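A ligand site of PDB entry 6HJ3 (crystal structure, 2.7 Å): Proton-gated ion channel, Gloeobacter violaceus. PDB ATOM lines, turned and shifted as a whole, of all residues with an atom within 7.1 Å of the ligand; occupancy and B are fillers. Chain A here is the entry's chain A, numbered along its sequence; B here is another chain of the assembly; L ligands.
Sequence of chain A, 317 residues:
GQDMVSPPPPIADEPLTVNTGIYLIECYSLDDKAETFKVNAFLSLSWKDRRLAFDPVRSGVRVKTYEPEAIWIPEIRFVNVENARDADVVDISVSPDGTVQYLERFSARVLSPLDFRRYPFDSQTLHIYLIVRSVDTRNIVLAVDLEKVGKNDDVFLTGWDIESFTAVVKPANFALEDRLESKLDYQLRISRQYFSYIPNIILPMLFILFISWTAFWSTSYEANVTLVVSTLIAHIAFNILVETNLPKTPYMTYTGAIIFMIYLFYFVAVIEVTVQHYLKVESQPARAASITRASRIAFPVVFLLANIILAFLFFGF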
ATOM      1  N   GLU A  75     -24.442  21.794   4.901  1.00  0.00           N
ATOM      2  CA  GLU A  75     -23.518  20.715   5.272  1.00  0.00           C
ATOM      3  C   GLU A  75     -24.354  19.522   5.733  1.00  0.00           C
ATOM      4  O   GLU A  75     -24.772  19.467   6.902  1.00  0.00           O
ATOM      5  CB  GLU A  75     -22.581  21.139   6.417  1.00  0.00           C
ATOM      6  CG  GLU A  75     -21.438  22.065   6.026  1.00  0.00           C
ATOM      7  CD  GLU A  75     -20.574  22.498   7.203  1.00  0.00           C
ATOM      8  OE1 GLU A  75     -20.421  21.723   8.168  1.00  0.00           O
ATOM      9  OE2 GLU A  75     -20.000  23.610   7.121  1.00  0.00           O
ATOM     10  N   ILE A  76     -24.624  18.610   4.775  1.00  0.00           N
ATOM     11  CA  ILE A  76     -25.390  17.386   4.959  1.00  0.00           C
ATOM     12  C   ILE A  76     -24.408  16.210   5.155  1.00  0.00           C
ATOM     13  O   ILE A  76     -23.445  16.081   4.398  1.00  0.00           O
ATOM     14  CB  ILE A  76     -26.298  17.140   3.718  1.00  0.00           C
ATOM     15  CG1 ILE A  76     -27.319  18.281   3.494  1.00  0.00           C
ATOM     16  CG2 ILE A  76     -26.978  15.758   3.773  1.00  0.00           C
ATOM     17  CD1 ILE A  76     -28.509  18.440   4.471  1.00  0.00           C
ATOM     18  N   ARG A  77     -24.659  15.376   6.154  1.00  0.00           N
ATOM     19  CA  ARG A  77     -23.834  14.194   6.446  1.00  0.00           C
ATOM     20  C   ARG A  77     -24.704  12.997   6.685  1.00  0.00           C
ATOM     21  O   ARG A  77     -25.922  13.114   6.835  1.00  0.00           O
ATOM     22  CB  ARG A  77     -22.962  14.431   7.691  1.00  0.00           C
ATOM     23  CG  ARG A  77     -21.797  15.391   7.492  1.00  0.00           C
ATOM     24  CD  ARG A  77     -21.095  15.666   8.797  1.00  0.00           C
ATOM     25  NE  ARG A  77     -21.992  16.302   9.772  1.00  0.00           N
ATOM     26  CZ  ARG A  77     -22.245  17.596   9.803  1.00  0.00           C
ATOM     27  NH1 ARG A  77     -21.694  18.413   8.921  1.00  0.00           N
ATOM     28  NH2 ARG A  77     -23.072  18.091  10.713  1.00  0.00           N
ATOM     29  N   PHE A  78     -24.067  11.820   6.700  1.00  0.00           N
ATOM     30  CA  PHE A  78     -24.688  10.542   7.036  1.00  0.00           C
ATOM     31  C   PHE A  78     -24.247  10.195   8.428  1.00  0.00           C
ATOM     32  O   PHE A  78     -23.086  10.408   8.787  1.00  0.00           O
ATOM     33  CB  PHE A  78     -24.312   9.434   6.046  1.00  0.00           C
ATOM     34  CG  PHE A  78     -24.948   9.605   4.698  1.00  0.00           C
ATOM     35  CD1 PHE A  78     -26.295   9.362   4.514  1.00  0.00           C
ATOM     36  CD2 PHE A  78     -24.210  10.059   3.617  1.00  0.00           C
ATOM     37  CE1 PHE A  78     -26.901   9.549   3.263  1.00  0.00           C
ATOM     38  CE2 PHE A  78     -24.817  10.254   2.381  1.00  0.00           C
ATOM     39  CZ  PHE A  78     -26.159  10.008   2.206  1.00  0.00           C
ATOM     40  N   VAL A  79     -25.173   9.703   9.227  1.00  0.00           N
ATOM     41  CA  VAL A  79     -24.838   9.353  10.605  1.00  0.00           C
ATOM     42  C   VAL A  79     -24.011   8.042  10.646  1.00  0.00           C
ATOM     43  O   VAL A  79     -22.882   8.038  11.148  1.00  0.00           O
ATOM     44  CB  VAL A  79     -26.100   9.261  11.506  1.00  0.00           C
ATOM     45  CG1 VAL A  79     -25.713   9.060  12.968  1.00  0.00           C
ATOM     46  CG2 VAL A  79     -26.967  10.494  11.375  1.00  0.00           C
ATOM     47  N   ILE A 131     -28.416  13.573   8.064  1.00  0.00           N
ATOM     48  CA  ILE A 131     -28.428  14.547   9.164  1.00  0.00           C
ATOM     49  C   ILE A 131     -27.937  15.956   8.707  1.00  0.00           C
ATOM     50  O   ILE A 131     -27.159  16.074   7.758  1.00  0.00           O
ATOM     51  CB  ILE A 131     -27.648  13.972  10.395  1.00  0.00           C
ATOM     52  CG1 ILE A 131     -28.057  14.693  11.706  1.00  0.00           C
ATOM     53  CG2 ILE A 131     -26.118  13.927  10.194  1.00  0.00           C
ATOM     54  CD1 ILE A 131     -28.177  13.827  12.884  1.00  0.00           C
ATOM     55  N   VAL A 132     -28.460  17.008   9.375  1.00  0.00           N
ATOM     56  CA  VAL A 132     -28.068  18.398   9.169  1.00  0.00           C
ATOM     57  C   VAL A 132     -27.884  19.069  10.519  1.00  0.00           C
ATOM     58  O   VAL A 132     -28.695  18.861  11.430  1.00  0.00           O
ATOM     59  CB  VAL A 132     -28.946  19.203   8.172  1.00  0.00           C
ATOM     60  CG1 VAL A 132     -30.271  19.641   8.796  1.00  0.00           C
ATOM     61  CG2 VAL A 132     -28.179  20.412   7.635  1.00  0.00           C
ATOM     62  N   ARG A 133     -26.806  19.830  10.655  1.00  0.00           N
ATOM     63  CA  ARG A 133     -26.560  20.552  11.894  1.00  0.00           C
ATOM     64  C   ARG A 133     -26.935  22.029  11.723  1.00  0.00           C
ATOM     65  O   ARG A 133     -26.394  22.692  10.826  1.00  0.00           O
ATOM     66  CB  ARG A 133     -25.124  20.378  12.393  1.00  0.00           C
ATOM     67  CG  ARG A 133     -24.944  20.938  13.777  1.00  0.00           C
ATOM     68  CD  ARG A 133     -23.650  20.483  14.384  1.00  0.00           C
ATOM     69  NE  ARG A 133     -23.283  21.331  15.518  1.00  0.00           N
ATOM     70  CZ  ARG A 133     -23.555  21.028  16.780  1.00  0.00           C
ATOM     71  NH1 ARG A 133     -24.198  19.913  17.079  1.00  0.00           N
ATOM     72  NH2 ARG A 133     -23.160  21.838  17.764  1.00  0.00           N
ATOM     73  N   PHE A 174     -33.437  16.898  17.285  1.00  0.00           N
ATOM     74  CA  PHE A 174     -32.882  16.765  18.643  1.00  0.00           C
ATOM     75  C   PHE A 174     -31.730  17.707  18.887  1.00  0.00           C
ATOM     76  O   PHE A 174     -31.106  18.189  17.939  1.00  0.00           O
ATOM     77  CB  PHE A 174     -32.457  15.313  18.939  1.00  0.00           C
ATOM     78  CG  PHE A 174     -31.333  14.806  18.065  1.00  0.00           C
ATOM     79  CD1 PHE A 174     -30.016  14.832  18.510  1.00  0.00           C
ATOM     80  CD2 PHE A 174     -31.585  14.307  16.791  1.00  0.00           C
ATOM     81  CE1 PHE A 174     -28.977  14.377  17.690  1.00  0.00           C
ATOM     82  CE2 PHE A 174     -30.555  13.888  15.964  1.00  0.00           C
ATOM     83  CZ  PHE A 174     -29.257  13.908  16.418  1.00  0.00           C
ATOM     84  N   LEU A 176     -27.950  18.399  20.180  1.00  0.00           N
ATOM     85  CA  LEU A 176     -26.634  17.834  20.389  1.00  0.00           C
ATOM     86  C   LEU A 176     -25.629  18.978  20.439  1.00  0.00           C
ATOM     87  O   LEU A 176     -25.475  19.722  19.474  1.00  0.00           O
ATOM     88  CB  LEU A 176     -26.294  16.784  19.320  1.00  0.00           C
ATOM     89  CG  LEU A 176     -24.835  16.318  19.222  1.00  0.00           C
ATOM     90  CD1 LEU A 176     -24.376  15.680  20.523  1.00  0.00           C
ATOM     91  CD2 LEU A 176     -24.657  15.385  18.045  1.00  0.00           C
ATOM     92  N   GLU A 181     -30.196  19.356  15.536  1.00  0.00           N
ATOM     93  CA  GLU A 181     -29.862  18.422  14.489  1.00  0.00           C
ATOM     94  C   GLU A 181     -31.145  17.784  13.983  1.00  0.00           C
ATOM     95  O   GLU A 181     -31.976  17.377  14.785  1.00  0.00           O
ATOM     96  CB  GLU A 181     -28.924  17.359  15.049  1.00  0.00           C
ATOM     97  CG  GLU A 181     -27.655  17.234  14.221  1.00  0.00           C
ATOM     98  CD  GLU A 181     -26.358  17.452  14.962  1.00  0.00           C
ATOM     99  OE1 GLU A 181     -26.354  18.092  16.041  1.00  0.00           O
ATOM    100  OE2 GLU A 181     -25.314  17.048  14.397  1.00  0.00           O
ATOM    101  N   LYS A 183     -32.616  14.706  11.755  1.00  0.00           N
ATOM    102  CA  LYS A 183     -32.231  13.383  11.258  1.00  0.00           C
ATOM    103  C   LYS A 183     -33.329  12.703  10.432  1.00  0.00           C
ATOM    104  O   LYS A 183     -34.489  12.746  10.834  1.00  0.00           O
ATOM    105  CB  LYS A 183     -31.820  12.500  12.461  1.00  0.00           C
ATOM    106  CG  LYS A 183     -31.104  11.185  12.119  1.00  0.00           C
ATOM    107  CD  LYS A 183     -30.716  10.478  13.410  1.00  0.00           C
ATOM    108  CE  LYS A 183     -31.486   9.197  13.684  1.00  0.00           C
ATOM    109  NZ  LYS A 183     -32.865   9.396  14.179  1.00  0.00           N
ATOM    110  N   TYR B  23     -17.077  13.338  20.974  1.00  0.00           N
ATOM    111  CA  TYR B  23     -18.434  12.792  21.021  1.00  0.00           C
ATOM    112  C   TYR B  23     -18.480  11.675  19.997  1.00  0.00           C
ATOM    113  O   TYR B  23     -18.520  11.990  18.792  1.00  0.00           O
ATOM    114  CB  TYR B  23     -19.523  13.876  20.767  1.00  0.00           C
ATOM    115  CG  TYR B  23     -20.938  13.343  20.851  1.00  0.00           C
ATOM    116  CD1 TYR B  23     -21.614  13.294  22.068  1.00  0.00           C
ATOM    117  CD2 TYR B  23     -21.573  12.811  19.728  1.00  0.00           C
ATOM    118  CE1 TYR B  23     -22.905  12.761  22.156  1.00  0.00           C
ATOM    119  CE2 TYR B  23     -22.863  12.257  19.807  1.00  0.00           C
ATOM    120  CZ  TYR B  23     -23.521  12.234  21.024  1.00  0.00           C
ATOM    121  OH  TYR B  23     -24.796  11.705  21.116  1.00  0.00           O
ATOM    122  N   LEU B  24     -18.457  10.380  20.439  1.00  0.00           N
ATOM    123  CA  LEU B  24     -18.482   9.209  19.564  1.00  0.00           C
ATOM    124  C   LEU B  24     -19.802   9.061  18.837  1.00  0.00           C
ATOM    125  O   LEU B  24     -20.880   9.070  19.457  1.00  0.00           O
ATOM    126  CB  LEU B  24     -18.197   7.909  20.326  1.00  0.00           C
ATOM    127  CG  LEU B  24     -16.997   7.880  21.272  1.00  0.00           C
ATOM    128  CD1 LEU B  24     -17.025   6.617  22.136  1.00  0.00           C
ATOM    129  CD2 LEU B  24     -15.672   7.981  20.506  1.00  0.00           C
ATOM    130  N   ILE B  25     -19.713   8.879  17.524  1.00  0.00           N
ATOM    131  CA  ILE B  25     -20.875   8.668  16.651  1.00  0.00           C
ATOM    132  C   ILE B  25     -20.915   7.182  16.269  1.00  0.00           C
ATOM    133  O   ILE B  25     -21.923   6.518  16.489  1.00  0.00           O
ATOM    134  CB  ILE B  25     -20.834   9.623  15.429  1.00  0.00           C
ATOM    135  CG1 ILE B  25     -20.956  11.098  15.885  1.00  0.00           C
ATOM    136  CG2 ILE B  25     -21.904   9.235  14.406  1.00  0.00           C
ATOM    137  CD1 ILE B  25     -20.027  12.056  15.240  1.00  0.00           C
ATOM    138  N   GLU B  26     -19.783   6.680  15.728  1.00  0.00           N
ATOM    139  CA  GLU B  26     -19.617   5.275  15.333  1.00  0.00           C
ATOM    140  C   GLU B  26     -18.366   4.682  15.963  1.00  0.00           C
ATOM    141  O   GLU B  26     -17.297   5.281  15.938  1.00  0.00           O
ATOM    142  CB  GLU B  26     -19.617   5.099  13.785  1.00  0.00           C
ATOM    143  CG  GLU B  26     -20.942   5.338  13.057  1.00  0.00           C
ATOM    144  CD  GLU B  26     -22.134   4.501  13.471  1.00  0.00           C
ATOM    145  OE1 GLU B  26     -21.956   3.329  13.884  1.00  0.00           O
ATOM    146  OE2 GLU B  26     -23.266   5.023  13.397  1.00  0.00           O
ATOM    147  N   ASN B  40     -15.472   7.094  14.616  1.00  0.00           N
ATOM    148  CA  ASN B  40     -16.079   8.201  13.877  1.00  0.00           C
ATOM    149  C   ASN B  40     -16.692   9.067  14.946  1.00  0.00           C
ATOM    150  O   ASN B  40     -17.545   8.620  15.710  1.00  0.00           O
ATOM    151  CB  ASN B  40     -17.106   7.714  12.843  1.00  0.00           C
ATOM    152  CG  ASN B  40     -17.429   8.798  11.855  1.00  0.00           C
ATOM    153  OD1 ASN B  40     -18.036   9.795  12.202  1.00  0.00           O
ATOM    154  ND2 ASN B  40     -16.976   8.647  10.629  1.00  0.00           N
ATOM    155  N   PHE B  42     -17.101  13.399  16.830  1.00  0.00           N
ATOM    156  CA  PHE B  42     -16.991  14.859  16.782  1.00  0.00           C
ATOM    157  C   PHE B  42     -15.805  15.233  17.652  1.00  0.00           C
ATOM    158  O   PHE B  42     -15.632  14.666  18.741  1.00  0.00           O
ATOM    159  CB  PHE B  42     -18.242  15.570  17.344  1.00  0.00           C
ATOM    160  CG  PHE B  42     -19.354  15.877  16.355  1.00  0.00           C
ATOM    161  CD1 PHE B  42     -19.063  16.266  15.054  1.00  0.00           C
ATOM    162  CD2 PHE B  42     -20.691  15.791  16.737  1.00  0.00           C
ATOM    163  CE1 PHE B  42     -20.098  16.521  14.148  1.00  0.00           C
ATOM    164  CE2 PHE B  42     -21.712  16.063  15.829  1.00  0.00           C
ATOM    165  CZ  PHE B  42     -21.408  16.413  14.543  1.00  0.00           C
ATOM    166  N   VAL B  90     -16.913  21.131  10.692  1.00  0.00           N
ATOM    167  CA  VAL B  90     -18.374  21.309  10.723  1.00  0.00           C
ATOM    168  C   VAL B  90     -18.668  22.803  10.921  1.00  0.00           C
ATOM    169  O   VAL B  90     -19.457  23.386  10.165  1.00  0.00           O
ATOM    170  CB  VAL B  90     -19.059  20.400  11.790  1.00  0.00           C
ATOM    171  CG1 VAL B  90     -20.554  20.691  11.916  1.00  0.00           C
ATOM    172  CG2 VAL B  90     -18.835  18.918  11.479  1.00  0.00           C
ATOM    173  N   ARG B 105     -15.786  16.710  12.344  1.00  0.00           N
ATOM    174  CA  ARG B 105     -16.138  15.302  12.449  1.00  0.00           C
ATOM    175  C   ARG B 105     -14.984  14.518  11.818  1.00  0.00           C
ATOM    176  O   ARG B 105     -14.580  14.806  10.693  1.00  0.00           O
ATOM    177  CB  ARG B 105     -17.506  14.958  11.833  1.00  0.00           C
ATOM    178  CG  ARG B 105     -18.056  13.626  12.338  1.00  0.00           C
ATOM    179  CD  ARG B 105     -19.413  13.349  11.752  1.00  0.00           C
ATOM    180  NE  ARG B 105     -19.679  11.910  11.738  1.00  0.00           N
ATOM    181  CZ  ARG B 105     -20.633  11.298  11.037  1.00  0.00           C
ATOM    182  NH1 ARG B 105     -21.466  11.993  10.286  1.00  0.00           N
ATOM    183  NH2 ARG B 105     -20.765   9.984  11.091  1.00  0.00           N
ATOM    184  N   ASN B 152     -23.254   8.575  21.268  1.00  0.00           N
ATOM    185  CA  ASN B 152     -24.695   8.386  21.144  1.00  0.00           C
ATOM    186  C   ASN B 152     -25.119   6.992  21.510  1.00  0.00           C
ATOM    187  O   ASN B 152     -24.274   6.108  21.647  1.00  0.00           O
ATOM    188  CB  ASN B 152     -25.323   8.860  19.829  1.00  0.00           C
ATOM    189  CG  ASN B 152     -24.674   8.457  18.548  1.00  0.00           C
ATOM    190  OD1 ASN B 152     -24.704   7.291  18.156  1.00  0.00           O
ATOM    191  ND2 ASN B 152     -24.277   9.456  17.792  1.00  0.00           N
ATOM    192  N   ASP B 154     -26.952   4.800  19.789  1.00  0.00           N
ATOM    193  CA  ASP B 154     -26.694   3.969  18.605  1.00  0.00           C
ATOM    194  C   ASP B 154     -25.295   3.305  18.600  1.00  0.00           C
ATOM    195  O   ASP B 154     -25.158   2.253  17.954  1.00  0.00           O
ATOM    196  CB  ASP B 154     -26.876   4.801  17.305  1.00  0.00           C
ATOM    197  CG  ASP B 154     -28.286   5.303  17.029  1.00  0.00           C
ATOM    198  OD1 ASP B 154     -29.257   4.560  17.320  1.00  0.00           O
ATOM    199  OD2 ASP B 154     -28.423   6.431  16.470  1.00  0.00           O
HETATM  200  O1  LIG L   1     -24.418  11.567  15.626  1.00  0.00           O
HETATM  201  C1  LIG L   1     -25.052  12.572  15.356  1.00  0.00           C
HETATM  202  O2  LIG L   1     -26.131  12.873  16.095  1.00  0.00           O
HETATM  203  C2  LIG L   1     -24.777  13.607  14.321  1.00  0.00           C
HETATM  204  C3  LIG L   1     -23.765  13.492  13.446  1.00  0.00           C
HETATM  205  C4  LIG L   1     -23.535  14.586  12.469  1.00  0.00           C
HETATM  206  O3  LIG L   1     -24.104  15.663  12.333  1.00  0.00           O
HETATM  207  O4  LIG L   1     -22.508  14.293  11.666  1.00  0.00           O
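The side-chain amide nitrogen (ND2) of Asn 152 of chain B sits at hydrogen-bond distance from an oxygen (O1) of the ligand, 3.0 Å away.
An oxygen (O4) of the ligand is in salt-bridge range of the guanidinium group of Arg 105 of chain B (2.9 Å).
The side-chain carboxylate of Glu 181 lies close to an oxygen (O3) of the ligand.
The guanidinium group (NE) of Arg 77 is in salt-bridge range of an oxygen (O4) of the ligand (2.8 Å).
OD1 of Asn 40 of chain B sits at hydrogen-bond distance from NE of Arg 105 of chain B, at 2.7 Å.
The side-chain hydroxyl (OH) of Tyr 23 of chain B sits close to the backbone NH (N) of Asn 152 of chain B, at 3.5 Å.
O of Val 79 is in hydrogen-bond range of NH2 of Arg 105 of chain B (2.9 Å).
The backbone carbonyl oxygen of Phe 174 is in hydrogen-bond range of the backbone NH of Glu 181 (2.8 Å).
The backbone NH of Ile 25 of chain B lies within hydrogen-bond range of the backbone carbonyl oxygen of Asn 40 of chain B (2.8 Å).
O of Leu 176 lies within hydrogen-bond range of NH1 of Arg 133 (2.7 Å).
N of Asn 152 of chain B is in hydrogen-bond range of O of Leu 24 of chain B, 3.0 Å away.
NH1 of Arg 77 is in salt-bridge range of OE1 of Glu 75 (3.6 Å).
Residues that only touch the ligand: Val 79, Ile 131, Phe 174, Leu 176, Ile 25 of chain B and Phe 42 of chain B.
Hydrophobic or aromatic side chains that line the ligand: Val 79, Ile 131, Phe 174, Leu 176, Ile 25 of chain B and Phe 42 of chain B.
Within 4 Å of the ligand: Arg 77, Val 79, Ile 131, Phe 174, Leu 176, Glu 181, Ile 25 of chain B, Phe 42 of chain B, Arg 105 of chain B and Asn 152 of chain B.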
